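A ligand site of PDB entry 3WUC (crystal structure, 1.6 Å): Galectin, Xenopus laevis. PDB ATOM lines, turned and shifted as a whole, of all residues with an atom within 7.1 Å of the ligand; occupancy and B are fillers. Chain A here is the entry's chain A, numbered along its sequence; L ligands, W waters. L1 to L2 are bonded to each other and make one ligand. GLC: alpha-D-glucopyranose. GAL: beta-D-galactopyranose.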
ATOM      1  N   MET A   3      18.771  -4.856  18.435  1.00  0.00           N
ATOM      2  CA  MET A   3      17.587  -4.593  19.307  1.00  0.00           C
ATOM      3  C   MET A   3      16.930  -5.938  19.662  1.00  0.00           C
ATOM      4  O   MET A   3      17.163  -6.939  18.969  1.00  0.00           O
ATOM      5  CB  MET A   3      16.624  -3.661  18.599  1.00  0.00           C
ATOM      6  CG  MET A   3      15.740  -4.352  17.544  1.00  0.00           C
ATOM      7  SD  MET A   3      14.281  -3.475  16.945  1.00  0.00           S
ATOM      8  CE  MET A   3      13.925  -4.555  15.566  1.00  0.00           C
ATOM      9  N   ASP A   4      16.094  -5.995  20.710  1.00  0.00           N
ATOM     10  CA  ASP A   4      15.424  -7.267  21.074  1.00  0.00           C
ATOM     11  C   ASP A   4      14.126  -7.564  20.324  1.00  0.00           C
ATOM     12  O   ASP A   4      13.738  -8.689  20.151  1.00  0.00           O
ATOM     13  CB  ASP A   4      15.088  -7.360  22.581  1.00  0.00           C
ATOM     14  CG  ASP A   4      14.225  -6.216  23.082  1.00  0.00           C
ATOM     15  OD1 ASP A   4      14.258  -5.230  22.406  1.00  0.00           O
ATOM     16  OD2 ASP A   4      13.544  -6.266  24.104  1.00  0.00           O
ATOM     17  N   MET A   5      13.404  -6.529  19.921  1.00  0.00           N
ATOM     18  CA  MET A   5      12.112  -6.708  19.328  1.00  0.00           C
ATOM     19  C   MET A   5      12.182  -7.369  17.939  1.00  0.00           C
ATOM     20  O   MET A   5      13.168  -7.218  17.279  1.00  0.00           O
ATOM     21  CB  MET A   5      11.454  -5.295  19.118  1.00  0.00           C
ATOM     22  CG  MET A   5      11.089  -4.577  20.399  1.00  0.00           C
ATOM     23  SD  MET A   5      10.255  -2.949  20.175  1.00  0.00           S
ATOM     24  CE  MET A   5      11.688  -2.013  19.614  1.00  0.00           C
ATOM     25  N   ARG A  34       7.042  -4.941  24.912  1.00  0.00           N
ATOM     26  CA  ARG A  34       6.960  -3.624  24.346  1.00  0.00           C
ATOM     27  C   ARG A  34       6.792  -3.759  22.837  1.00  0.00           C
ATOM     28  O   ARG A  34       7.139  -4.791  22.271  1.00  0.00           O
ATOM     29  CB  ARG A  34       8.192  -2.801  24.629  1.00  0.00           C
ATOM     30  CG  ARG A  34       9.448  -3.204  23.863  1.00  0.00           C
ATOM     31  CD  ARG A  34      10.695  -2.681  24.580  1.00  0.00           C
ATOM     32  NE  ARG A  34      11.972  -3.007  23.887  1.00  0.00           N
ATOM     33  CZ  ARG A  34      12.771  -2.097  23.347  1.00  0.00           C
ATOM     34  NH1 ARG A  34      12.492  -0.804  23.240  1.00  0.00           N
ATOM     35  NH2 ARG A  34      13.908  -2.522  22.795  1.00  0.00           N
ATOM     36  N   ALA A  36       6.993  -0.970  19.037  1.00  0.00           N
ATOM     37  CA  ALA A  36       7.293   0.340  18.580  1.00  0.00           C
ATOM     38  C   ALA A  36       6.876   0.583  17.162  1.00  0.00           C
ATOM     39  O   ALA A  36       6.825  -0.363  16.353  1.00  0.00           O
ATOM     40  CB  ALA A  36       8.793   0.518  18.586  1.00  0.00           C
ATOM     41  N   HIS A  49      10.466   7.648  17.523  1.00  0.00           N
ATOM     42  CA  HIS A  49      10.406   6.270  18.022  1.00  0.00           C
ATOM     43  C   HIS A  49       9.379   6.251  19.097  1.00  0.00           C
ATOM     44  O   HIS A  49       9.496   6.880  20.144  1.00  0.00           O
ATOM     45  CB  HIS A  49      11.756   5.878  18.570  1.00  0.00           C
ATOM     46  CG  HIS A  49      11.809   4.608  19.351  1.00  0.00           C
ATOM     47  ND1 HIS A  49      11.746   3.331  18.835  1.00  0.00           N
ATOM     48  CD2 HIS A  49      12.027   4.404  20.694  1.00  0.00           C
ATOM     49  CE1 HIS A  49      11.935   2.417  19.777  1.00  0.00           C
ATOM     50  NE2 HIS A  49      12.134   3.054  20.913  1.00  0.00           N
ATOM     51  N   ASN A  51       7.312   4.084  21.520  1.00  0.00           N
ATOM     52  CA  ASN A  51       7.606   2.793  22.124  1.00  0.00           C
ATOM     53  C   ASN A  51       6.809   2.430  23.396  1.00  0.00           C
ATOM     54  O   ASN A  51       7.248   2.621  24.540  1.00  0.00           O
ATOM     55  CB  ASN A  51       9.099   2.713  22.455  1.00  0.00           C
ATOM     56  CG  ASN A  51       9.581   1.319  22.899  1.00  0.00           C
ATOM     57  OD1 ASN A  51      10.487   1.256  23.777  1.00  0.00           O
ATOM     58  ND2 ASN A  51       8.941   0.209  22.467  1.00  0.00           N
ATOM     59  N   ARG A  53       5.684   0.477  26.403  1.00  0.00           N
ATOM     60  CA  ARG A  53       6.259  -0.577  27.188  1.00  0.00           C
ATOM     61  C   ARG A  53       5.292  -1.064  28.226  1.00  0.00           C
ATOM     62  O   ARG A  53       4.871  -0.330  29.126  1.00  0.00           O
ATOM     63  CB  ARG A  53       7.468  -0.003  27.855  1.00  0.00           C
ATOM     64  CG  ARG A  53       8.571   0.413  26.880  1.00  0.00           C
ATOM     65  CD  ARG A  53       9.722   1.188  27.557  1.00  0.00           C
ATOM     66  NE  ARG A  53      10.778   1.435  26.558  1.00  0.00           N
ATOM     67  CZ  ARG A  53      12.030   1.828  26.836  1.00  0.00           C
ATOM     68  NH1 ARG A  53      12.339   1.967  28.085  1.00  0.00           N
ATOM     69  NH2 ARG A  53      12.897   1.972  25.872  1.00  0.00           N
ATOM     70  N   TYR A  56       9.538  -2.817  30.476  1.00  0.00           N
ATOM     71  CA  TYR A  56      10.908  -2.849  29.989  1.00  0.00           C
ATOM     72  C   TYR A  56      11.681  -1.807  30.696  1.00  0.00           C
ATOM     73  O   TYR A  56      11.279  -0.633  30.824  1.00  0.00           O
ATOM     74  CB  TYR A  56      10.944  -2.578  28.450  1.00  0.00           C
ATOM     75  CG  TYR A  56      12.296  -2.679  27.777  1.00  0.00           C
ATOM     76  CD1 TYR A  56      12.789  -3.935  27.385  1.00  0.00           C
ATOM     77  CD2 TYR A  56      13.037  -1.557  27.519  1.00  0.00           C
ATOM     78  CE1 TYR A  56      14.005  -3.988  26.794  1.00  0.00           C
ATOM     79  CE2 TYR A  56      14.295  -1.630  26.904  1.00  0.00           C
ATOM     80  CZ  TYR A  56      14.739  -2.846  26.532  1.00  0.00           C
ATOM     81  OH  TYR A  56      15.998  -2.896  25.935  1.00  0.00           O
ATOM     82  N   SER A  57      12.921  -2.149  31.014  1.00  0.00           N
ATOM     83  CA  SER A  57      13.724  -1.272  31.825  1.00  0.00           C
ATOM     84  C   SER A  57      12.987  -0.870  33.100  1.00  0.00           C
ATOM     85  O   SER A  57      12.261  -1.689  33.635  1.00  0.00           O
ATOM     86  CB  SER A  57      14.272  -0.072  31.032  1.00  0.00           C
ATOM     87  OG  SER A  57      15.225   0.680  31.813  1.00  0.00           O
ATOM     88  N   VAL A  58      13.030   0.422  33.460  1.00  0.00           N
ATOM     89  CA  VAL A  58      12.316   0.863  34.660  1.00  0.00           C
ATOM     90  C   VAL A  58      10.849   1.185  34.353  1.00  0.00           C
ATOM     91  O   VAL A  58      10.133   1.620  35.220  1.00  0.00           O
ATOM     92  CB  VAL A  58      12.949   2.156  35.180  1.00  0.00           C
ATOM     93  CG1 VAL A  58      14.353   1.856  35.702  1.00  0.00           C
ATOM     94  CG2 VAL A  58      12.965   3.246  34.135  1.00  0.00           C
ATOM     95  N   ASP A  59      10.412   1.004  33.116  1.00  0.00           N
ATOM     96  CA  ASP A  59       9.066   1.390  32.702  1.00  0.00           C
ATOM     97  C   ASP A  59       8.034   0.297  32.694  1.00  0.00           C
ATOM     98  O   ASP A  59       8.243  -0.776  32.139  1.00  0.00           O
ATOM     99  CB  ASP A  59       9.160   2.012  31.287  1.00  0.00           C
ATOM    100  CG  ASP A  59      10.149   3.125  31.247  1.00  0.00           C
ATOM    101  OD1 ASP A  59      10.049   4.092  32.069  1.00  0.00           O
ATOM    102  OD2 ASP A  59      11.089   2.991  30.426  1.00  0.00           O
ATOM    103  N   VAL A  64       7.407   5.327  25.972  1.00  0.00           N
ATOM    104  CA  VAL A  64       8.642   6.125  25.763  1.00  0.00           C
ATOM    105  C   VAL A  64       8.633   6.637  24.331  1.00  0.00           C
ATOM    106  O   VAL A  64       8.379   5.815  23.396  1.00  0.00           O
ATOM    107  CB  VAL A  64       9.864   5.219  26.007  1.00  0.00           C
ATOM    108  CG1 VAL A  64      11.166   5.792  25.408  1.00  0.00           C
ATOM    109  CG2 VAL A  64      10.010   4.886  27.481  1.00  0.00           C
ATOM    110  N   LEU A  65       8.862   7.922  24.205  1.00  0.00           N
ATOM    111  CA  LEU A  65       9.127   8.531  22.880  1.00  0.00           C
ATOM    112  C   LEU A  65      10.583   8.951  22.820  1.00  0.00           C
ATOM    113  O   LEU A  65      11.134   9.506  23.809  1.00  0.00           O
ATOM    114  CB  LEU A  65       8.257   9.778  22.658  1.00  0.00           C
ATOM    115  CG  LEU A  65       6.737   9.488  22.715  1.00  0.00           C
ATOM    116  CD1 LEU A  65       6.027  10.818  22.601  1.00  0.00           C
ATOM    117  CD2 LEU A  65       6.272   8.661  21.567  1.00  0.00           C
ATOM    118  N   ASN A  66      11.260   8.798  21.702  1.00  0.00           N
ATOM    119  CA  ASN A  66      12.615   9.279  21.524  1.00  0.00           C
ATOM    120  C   ASN A  66      12.906   9.522  20.034  1.00  0.00           C
ATOM    121  O   ASN A  66      12.116   9.216  19.173  1.00  0.00           O
ATOM    122  CB  ASN A  66      13.628   8.353  22.155  1.00  0.00           C
ATOM    123  CG  ASN A  66      14.868   9.072  22.614  1.00  0.00           C
ATOM    124  OD1 ASN A  66      15.091  10.238  22.320  1.00  0.00           O
ATOM    125  ND2 ASN A  66      15.704   8.327  23.297  1.00  0.00           N
ATOM    126  N   SER A  67      14.035  10.145  19.766  1.00  0.00           N
ATOM    127  CA  SER A  67      14.603  10.352  18.470  1.00  0.00           C
ATOM    128  C   SER A  67      16.013   9.713  18.416  1.00  0.00           C
ATOM    129  O   SER A  67      16.593   9.469  19.466  1.00  0.00           O
ATOM    130  CB  SER A  67      14.693  11.817  18.064  1.00  0.00           C
ATOM    131  OG  SER A  67      15.315  12.533  19.131  1.00  0.00           O
ATOM    132  N   TRP A  73      20.703   7.413  20.374  1.00  0.00           N
ATOM    133  CA  TRP A  73      19.405   7.814  20.975  1.00  0.00           C
ATOM    134  C   TRP A  73      19.563   9.187  21.650  1.00  0.00           C
ATOM    135  O   TRP A  73      20.597   9.502  22.332  1.00  0.00           O
ATOM    136  CB  TRP A  73      18.964   6.787  21.990  1.00  0.00           C
ATOM    137  CG  TRP A  73      18.505   5.524  21.402  1.00  0.00           C
ATOM    138  CD1 TRP A  73      19.143   4.299  21.456  1.00  0.00           C
ATOM    139  CD2 TRP A  73      17.345   5.315  20.604  1.00  0.00           C
ATOM    140  NE1 TRP A  73      18.417   3.346  20.783  1.00  0.00           N
ATOM    141  CE2 TRP A  73      17.315   3.950  20.244  1.00  0.00           C
ATOM    142  CE3 TRP A  73      16.319   6.154  20.175  1.00  0.00           C
ATOM    143  CZ2 TRP A  73      16.280   3.406  19.510  1.00  0.00           C
ATOM    144  CZ3 TRP A  73      15.329   5.598  19.386  1.00  0.00           C
ATOM    145  CH2 TRP A  73      15.303   4.250  19.095  1.00  0.00           C
ATOM    146  N   ASP A  74      18.564  10.024  21.508  1.00  0.00           N
ATOM    147  CA  ASP A  74      18.441  11.298  22.238  1.00  0.00           C
ATOM    148  C   ASP A  74      17.833  11.049  23.657  1.00  0.00           C
ATOM    149  O   ASP A  74      17.923   9.939  24.188  1.00  0.00           O
ATOM    150  CB  ASP A  74      17.697  12.305  21.371  1.00  0.00           C
ATOM    151  CG  ASP A  74      18.443  12.676  20.113  1.00  0.00           C
ATOM    152  OD1 ASP A  74      19.701  12.808  20.151  1.00  0.00           O
ATOM    153  OD2 ASP A  74      17.839  12.755  19.010  1.00  0.00           O
ATOM    154  N   ILE A  75      17.289  12.092  24.273  1.00  0.00           N
ATOM    155  CA  ILE A  75      16.728  11.968  25.589  1.00  0.00           C
ATOM    156  C   ILE A  75      15.262  11.527  25.539  1.00  0.00           C
ATOM    157  O   ILE A  75      14.461  12.146  24.865  1.00  0.00           O
ATOM    158  CB  ILE A  75      16.905  13.281  26.386  1.00  0.00           C
ATOM    159  CG1 ILE A  75      18.441  13.517  26.590  1.00  0.00           C
ATOM    160  CG2 ILE A  75      16.277  13.140  27.748  1.00  0.00           C
ATOM    161  CD1 ILE A  75      18.835  14.901  26.275  1.00  0.00           C
ATOM    162  N   GLU A  76      14.942  10.449  26.238  1.00  0.00           N
ATOM    163  CA  GLU A  76      13.577   9.924  26.279  1.00  0.00           C
ATOM    164  C   GLU A  76      12.575  10.865  26.892  1.00  0.00           C
ATOM    165  O   GLU A  76      12.854  11.585  27.863  1.00  0.00           O
ATOM    166  CB  GLU A  76      13.495   8.620  27.050  1.00  0.00           C
ATOM    167  CG  GLU A  76      14.246   7.518  26.431  1.00  0.00           C
ATOM    168  CD  GLU A  76      14.376   6.298  27.295  1.00  0.00           C
ATOM    169  OE1 GLU A  76      13.944   6.274  28.480  1.00  0.00           O
ATOM    170  OE2 GLU A  76      14.942   5.353  26.770  1.00  0.00           O
ATOM    171  N   LYS A  77      11.410  10.973  26.297  1.00  0.00           N
ATOM    172  CA  LYS A  77      10.208  11.585  26.901  1.00  0.00           C
ATOM    173  C   LYS A  77       9.180  10.509  27.226  1.00  0.00           C
ATOM    174  O   LYS A  77       9.034   9.501  26.476  1.00  0.00           O
ATOM    175  CB  LYS A  77       9.617  12.557  25.902  1.00  0.00           C
ATOM    176  CG  LYS A  77      10.378  13.826  25.627  1.00  0.00           C
ATOM    177  CD  LYS A  77       9.820  14.956  26.545  1.00  0.00           C
ATOM    178  CE  LYS A  77      10.549  16.276  26.423  1.00  0.00           C
ATOM    179  NZ  LYS A  77      10.105  17.375  27.377  1.00  0.00           N
ATOM    180  N   LYS A  78       8.496  10.624  28.369  1.00  0.00           N
ATOM    181  CA  LYS A  78       7.659   9.499  28.749  1.00  0.00           C
ATOM    182  C   LYS A  78       6.223  10.009  29.080  1.00  0.00           C
ATOM    183  O   LYS A  78       6.075  11.108  29.658  1.00  0.00           O
ATOM    184  CB  LYS A  78       8.149   8.874  30.010  1.00  0.00           C
ATOM    185  CG  LYS A  78       9.586   8.351  29.935  1.00  0.00           C
ATOM    186  CD  LYS A  78       9.968   7.485  31.093  1.00  0.00           C
ATOM    187  CE  LYS A  78      11.417   7.026  30.970  1.00  0.00           C
ATOM    188  NZ  LYS A  78      11.688   6.188  32.154  1.00  0.00           N
HETATM  189  C1  GLC L   1      18.105   2.803  29.771  1.00  0.00           C
HETATM  190  C2  GLC L   1      16.620   3.205  29.522  1.00  0.00           C
HETATM  191  C3  GLC L   1      16.125   2.348  28.344  1.00  0.00           C
HETATM  192  C4  GLC L   1      17.082   2.261  27.154  1.00  0.00           C
HETATM  193  C5  GLC L   1      18.341   1.585  27.677  1.00  0.00           C
HETATM  194  C6  GLC L   1      19.339   1.202  26.609  1.00  0.00           C
HETATM  195  O1  GLC L   1      17.874   1.553  30.308  1.00  0.00           O
HETATM  196  O2  GLC L   1      15.759   3.076  30.627  1.00  0.00           O
HETATM  197  O3  GLC L   1      14.959   2.986  27.865  1.00  0.00           O
HETATM  198  O4  GLC L   1      16.532   1.314  26.194  1.00  0.00           O
HETATM  199  O5  GLC L   1      18.909   2.393  28.687  1.00  0.00           O
HETATM  200  O6  GLC L   1      19.903   2.426  26.240  1.00  0.00           O
HETATM  201  C1  GAL L   2      16.560   1.687  24.834  1.00  0.00           C
HETATM  202  C2  GAL L   2      16.098   0.487  23.986  1.00  0.00           C
HETATM  203  C3  GAL L   2      15.786   0.917  22.554  1.00  0.00           C
HETATM  204  C4  GAL L   2      14.920   2.205  22.521  1.00  0.00           C
HETATM  205  C5  GAL L   2      15.541   3.257  23.414  1.00  0.00           C
HETATM  206  C6  GAL L   2      14.720   4.545  23.435  1.00  0.00           C
HETATM  207  O2  GAL L   2      17.021  -0.632  24.054  1.00  0.00           O
HETATM  208  O3  GAL L   2      15.267  -0.164  21.796  1.00  0.00           O
HETATM  209  O4  GAL L   2      13.572   1.876  22.883  1.00  0.00           O
HETATM  210  O5  GAL L   2      15.632   2.743  24.742  1.00  0.00           O
HETATM  211  O6  GAL L   2      15.335   5.572  24.179  1.00  0.00           O
HETATM  212  O   HOH W   1      16.645   4.531  32.813  1.00  0.00           O
HETATM  213  O   HOH W   2      18.044   5.366  25.092  1.00  0.00           O
HETATM  214  O   HOH W   3      17.477  -2.352  21.904  1.00  0.00           O
HETATM  215  O   HOH W   4      13.518   4.404  30.421  1.00  0.00           O
HETATM  216  O   HOH W   5      19.695   1.056  32.384  1.00  0.00           O
HETATM  217  O   HOH W   6      19.628   0.027  23.037  1.00  0.00           O
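The side-chain carboxylate (OE2) of Glu 76 is in hydrogen-bond range of an oxygen (O3) of GLC L1 (2.6 Å). A ring nitrogen (NE2) of His 49 lies within hydrogen-bond range of an oxygen (O4) of GAL L2. The side-chain hydroxyl of Ser 57 lies within hydrogen-bond range of an oxygen (O2) of GLC L1, at 2.7 Å. The guanidinium group (NH1) of Arg 53 lies within hydrogen-bond range of an oxygen (O3) of GLC L1. NH2 of Arg 34 is in hydrogen-bond range of O3 of GAL L2. O6 of GAL L2 is in hydrogen-bond range of ND2 of Asn 66 (2.9 Å). An oxygen (O2) of GAL L2 lies within hydrogen-bond range of the side-chain hydroxyl (OH) of Tyr 56, 3.1 Å away. The side-chain amide oxygen (OD1) of Asn 51 lies within hydrogen-bond range of an oxygen (O4) of GAL L2, at 3.3 Å.
The backbone NH of His 49 is in hydrogen-bond range of the backbone carbonyl oxygen of Asn 66. OD1 of Asn 51 lies within hydrogen-bond range of NE of Arg 53, 2.8 Å away. The guanidinium group of Arg 53 lies within salt-bridge range of the side-chain carboxylate of Asp 59, at 2.8 Å. OD1 of Asn 51 sits at hydrogen-bond distance from NH1 of Arg 34 (2.9 Å). The guanidinium group (NH2) of Arg 34 is in salt-bridge range of the side-chain carboxylate (OD1) of Asp 4 (2.8 Å). The side-chain amide nitrogen (ND2) of Asn 66 is in hydrogen-bond range of the backbone carbonyl oxygen (O) of Asp 74 (2.9 Å). O of Ile 75 sits close to OD1 of Asn 66, 3.2 Å away. N of Asn 51 is in hydrogen-bond range of O of Val 64 (2.8 Å).
Residues that only touch the ligand: Trp 73 (3.5 Å). Hydrophobic or aromatic side chains that line the ligand: His 49, Tyr 56 and Trp 73. Within 4 Å of the ligand: Arg 34, His 49, Asn 51, Arg 53, Tyr 56, Ser 57, Asn 66, Trp 73 and Glu 76. Along chain A the residues within 4 Å of the ligand span positions 34 to 76. The nearest printed residue that does not touch the ligand is Val 64 (4.3 Å).
Water W4 lies within hydrogen-bond range of O2 of GLC L1, OE1 of Glu 76, OD2 of Asp 59 and NZ of Lys 78.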
